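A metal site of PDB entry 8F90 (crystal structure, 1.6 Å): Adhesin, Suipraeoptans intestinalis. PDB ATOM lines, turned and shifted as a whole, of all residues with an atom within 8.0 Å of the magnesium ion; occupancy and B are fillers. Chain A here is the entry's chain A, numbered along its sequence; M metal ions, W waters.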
ATOM      1  N   TYR A   5      20.862  33.882  28.667  1.00  0.00           N
ATOM      2  CA  TYR A   5      21.310  33.484  27.301  1.00  0.00           C
ATOM      3  C   TYR A   5      20.109  33.348  26.361  1.00  0.00           C
ATOM      4  O   TYR A   5      19.377  32.344  26.424  1.00  0.00           O
ATOM      5  CB  TYR A   5      22.131  32.186  27.292  1.00  0.00           C
ATOM      6  CG  TYR A   5      22.854  31.966  25.998  1.00  0.00           C
ATOM      7  CD1 TYR A   5      24.106  32.545  25.772  1.00  0.00           C
ATOM      8  CD2 TYR A   5      22.292  31.234  24.965  1.00  0.00           C
ATOM      9  CE1 TYR A   5      24.767  32.377  24.568  1.00  0.00           C
ATOM     10  CE2 TYR A   5      22.945  31.059  23.759  1.00  0.00           C
ATOM     11  CZ  TYR A   5      24.189  31.626  23.553  1.00  0.00           C
ATOM     12  OH  TYR A   5      24.850  31.465  22.370  1.00  0.00           O
ATOM     13  N   ASN A   7      18.875  32.520  22.784  1.00  0.00           N
ATOM     14  CA  ASN A   7      19.393  31.720  21.649  1.00  0.00           C
ATOM     15  C   ASN A   7      19.380  32.563  20.373  1.00  0.00           C
ATOM     16  O   ASN A   7      18.391  33.252  20.075  1.00  0.00           O
ATOM     17  CB  ASN A   7      18.605  30.433  21.432  1.00  0.00           C
ATOM     18  CG  ASN A   7      19.022  29.356  22.410  1.00  0.00           C
ATOM     19  OD1 ASN A   7      20.198  29.228  22.748  1.00  0.00           O
ATOM     20  ND2 ASN A   7      18.050  28.606  22.898  1.00  0.00           N
ATOM     21  N   ILE A 121      23.840  27.326  20.784  1.00  0.00           N
ATOM     22  CA  ILE A 121      22.395  27.086  21.080  1.00  0.00           C
ATOM     23  C   ILE A 121      22.284  26.343  22.418  1.00  0.00           C
ATOM     24  O   ILE A 121      22.896  25.270  22.557  1.00  0.00           O
ATOM     25  CB  ILE A 121      21.720  26.283  19.955  1.00  0.00           C
ATOM     26  CG1 ILE A 121      21.853  26.966  18.588  1.00  0.00           C
ATOM     27  CG2 ILE A 121      20.263  25.976  20.306  1.00  0.00           C
ATOM     28  CD1 ILE A 121      21.205  28.322  18.499  1.00  0.00           C
ATOM     29  N   ASP A 122      21.516  26.915  23.334  1.00  0.00           N
ATOM     30  CA  ASP A 122      21.131  26.265  24.612  1.00  0.00           C
ATOM     31  C   ASP A 122      19.871  25.438  24.348  1.00  0.00           C
ATOM     32  O   ASP A 122      18.817  26.036  24.118  1.00  0.00           O
ATOM     33  CB  ASP A 122      20.956  27.315  25.699  1.00  0.00           C
ATOM     34  CG  ASP A 122      20.620  26.721  27.056  1.00  0.00           C
ATOM     35  OD1 ASP A 122      20.926  25.524  27.290  1.00  0.00           O
ATOM     36  OD2 ASP A 122      20.059  27.468  27.866  1.00  0.00           O
ATOM     37  N   THR A 123      19.984  24.116  24.409  1.00  0.00           N
ATOM     38  CA  THR A 123      18.894  23.158  24.114  1.00  0.00           C
ATOM     39  C   THR A 123      18.141  22.776  25.389  1.00  0.00           C
ATOM     40  O   THR A 123      17.064  22.187  25.264  1.00  0.00           O
ATOM     41  CB  THR A 123      19.440  21.919  23.401  1.00  0.00           C
ATOM     42  OG1 THR A 123      20.253  21.188  24.333  1.00  0.00           O
ATOM     43  CG2 THR A 123      20.252  22.276  22.183  1.00  0.00           C
ATOM     44  N   ASP A 124      18.697  23.053  26.563  1.00  0.00           N
ATOM     45  CA  ASP A 124      18.189  22.493  27.840  1.00  0.00           C
ATOM     46  C   ASP A 124      17.909  23.585  28.872  1.00  0.00           C
ATOM     47  O   ASP A 124      17.558  23.211  30.002  1.00  0.00           O
ATOM     48  CB  ASP A 124      19.142  21.412  28.370  1.00  0.00           C
ATOM     49  CG  ASP A 124      20.607  21.808  28.478  1.00  0.00           C
ATOM     50  OD1 ASP A 124      20.938  23.008  28.330  1.00  0.00           O
ATOM     51  OD2 ASP A 124      21.417  20.884  28.703  1.00  0.00           O
ATOM     52  N   TYR A 125      18.035  24.873  28.508  1.00  0.00           N
ATOM     53  CA  TYR A 125      17.584  26.030  29.329  1.00  0.00           C
ATOM     54  C   TYR A 125      18.325  26.055  30.680  1.00  0.00           C
ATOM     55  O   TYR A 125      17.717  26.396  31.708  1.00  0.00           O
ATOM     56  CB  TYR A 125      16.056  25.998  29.469  1.00  0.00           C
ATOM     57  CG  TYR A 125      15.331  25.944  28.148  1.00  0.00           C
ATOM     58  CD1 TYR A 125      15.635  26.847  27.142  1.00  0.00           C
ATOM     59  CD2 TYR A 125      14.354  24.991  27.875  1.00  0.00           C
ATOM     60  CE1 TYR A 125      14.996  26.818  25.917  1.00  0.00           C
ATOM     61  CE2 TYR A 125      13.691  24.957  26.652  1.00  0.00           C
ATOM     62  CZ  TYR A 125      14.029  25.865  25.658  1.00  0.00           C
ATOM     63  OH  TYR A 125      13.411  25.855  24.440  1.00  0.00           O
ATOM     64  N   ASP A 126      19.625  25.715  30.663  1.00  0.00           N
ATOM     65  CA  ASP A 126      20.542  25.873  31.825  1.00  0.00           C
ATOM     66  C   ASP A 126      21.345  27.163  31.638  1.00  0.00           C
ATOM     67  O   ASP A 126      22.224  27.445  32.474  1.00  0.00           O
ATOM     68  CB  ASP A 126      21.425  24.627  31.997  1.00  0.00           C
ATOM     69  CG  ASP A 126      22.396  24.354  30.857  1.00  0.00           C
ATOM     70  OD1 ASP A 126      22.257  24.953  29.756  1.00  0.00           O
ATOM     71  OD2 ASP A 126      23.298  23.528  31.079  1.00  0.00           O
ATOM     72  N   ASN A 127      21.048  27.912  30.561  1.00  0.00           N
ATOM     73  CA  ASN A 127      21.670  29.196  30.175  1.00  0.00           C
ATOM     74  C   ASN A 127      23.081  28.951  29.624  1.00  0.00           C
ATOM     75  O   ASN A 127      23.806  29.935  29.420  1.00  0.00           O
ATOM     76  CB  ASN A 127      21.625  30.222  31.314  1.00  0.00           C
ATOM     77  CG  ASN A 127      20.328  31.021  31.275  1.00  0.00           C
ATOM     78  OD1 ASN A 127      19.230  30.471  31.193  1.00  0.00           O
ATOM     79  ND2 ASN A 127      20.475  32.323  31.284  1.00  0.00           N
ATOM     80  N   ILE A 128      23.425  27.686  29.362  1.00  0.00           N
ATOM     81  CA  ILE A 128      24.743  27.292  28.786  1.00  0.00           C
ATOM     82  C   ILE A 128      24.510  26.721  27.395  1.00  0.00           C
ATOM     83  O   ILE A 128      23.828  25.711  27.231  1.00  0.00           O
ATOM     84  CB  ILE A 128      25.480  26.283  29.700  1.00  0.00           C
ATOM     85  CG1 ILE A 128      25.668  26.837  31.106  1.00  0.00           C
ATOM     86  CG2 ILE A 128      26.810  25.885  29.054  1.00  0.00           C
ATOM     87  CD1 ILE A 128      26.160  25.811  32.098  1.00  0.00           C
ATOM     88  N   PRO A 129      25.048  27.381  26.348  1.00  0.00           N
ATOM     89  CA  PRO A 129      24.936  26.864  24.989  1.00  0.00           C
ATOM     90  C   PRO A 129      25.647  25.510  24.920  1.00  0.00           C
ATOM     91  O   PRO A 129      26.690  25.363  25.552  1.00  0.00           O
ATOM     92  CB  PRO A 129      25.577  27.940  24.090  1.00  0.00           C
ATOM     93  CG  PRO A 129      26.429  28.769  25.023  1.00  0.00           C
ATOM     94  CD  PRO A 129      25.812  28.642  26.407  1.00  0.00           C
ATOM     95  N   ASP A 130      25.047  24.554  24.213  1.00  0.00           N
ATOM     96  CA  ASP A 130      25.502  23.142  24.241  1.00  0.00           C
ATOM     97  C   ASP A 130      25.452  22.490  22.853  1.00  0.00           C
ATOM     98  O   ASP A 130      25.877  21.324  22.754  1.00  0.00           O
ATOM     99  CB  ASP A 130      24.690  22.394  25.308  1.00  0.00           C
ATOM    100  CG  ASP A 130      23.195  22.581  25.153  1.00  0.00           C
ATOM    101  OD1 ASP A 130      22.658  21.937  24.231  1.00  0.00           O
ATOM    102  OD2 ASP A 130      22.591  23.388  25.931  1.00  0.00           O
ATOM    103  N   THR A 131      24.982  23.178  21.799  1.00  0.00           N
ATOM    104  CA  THR A 131      24.983  22.607  20.414  1.00  0.00           C
ATOM    105  C   THR A 131      25.243  23.727  19.405  1.00  0.00           C
ATOM    106  O   THR A 131      24.916  24.884  19.661  1.00  0.00           O
ATOM    107  CB  THR A 131      23.701  21.830  20.116  1.00  0.00           C
ATOM    108  OG1 THR A 131      23.985  20.913  19.050  1.00  0.00           O
ATOM    109  CG2 THR A 131      22.524  22.696  19.730  1.00  0.00           C
HETATM  110 MG    MG M   1      22.456  24.269  27.810  1.00  0.00          MG
HETATM  111  O   HOH W   1      23.875  23.027  28.556  1.00  0.00           O
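The backbone NH of Tyr 125 sits close to the side-chain carboxylate of Asp 122, at 3.4 Å.
The side-chain carboxylate (OD2) of Asp 122 lies within hydrogen-bond range of the backbone NH (N) of Asn 127, at 2.9 Å.
The backbone NH (N) of Asp 122 is in hydrogen-bond range of the side-chain amide oxygen (OD1) of Asn 7 (2.7 Å).
OD1 of Asp 130 lies within hydrogen-bond range of OG1 of Thr 123, 2.5 Å away.
The backbone carbonyl oxygen (O) of Ile 121 sits at hydrogen-bond distance from the backbone NH (N) of Asp 130 (2.8 Å).
Within 4 Å of the magnesium ion: Asp 122, Asp 124, Asp 126, Ile 128 and Asp 130.
The nearest printed residue that does not touch the magnesium ion is Thr 123 (4.2 Å).
Water W1 binds the magnesium ion, 2.0 Å away.
The magnesium ion is bound by OD1 of Asp 124 (2.0 Å).
The side-chain carboxylate (OD1) of Asp 122 binds the magnesium ion.
The magnesium ion is bound by OD1 of Asp 126.
The magnesium ion is bound by the backbone carbonyl oxygen (O) of Ile 128 (2.1 Å).
OD2 of Asp 130 binds the magnesium ion (2.1 Å).
The magnesium ion has six donor atoms within binding distance.
Water W1 bridges the side-chain carboxylate (OD2) of Asp 126 (2.6 Å) and the side-chain carboxylate (OD2) of Asp 124 (3.3 Å).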
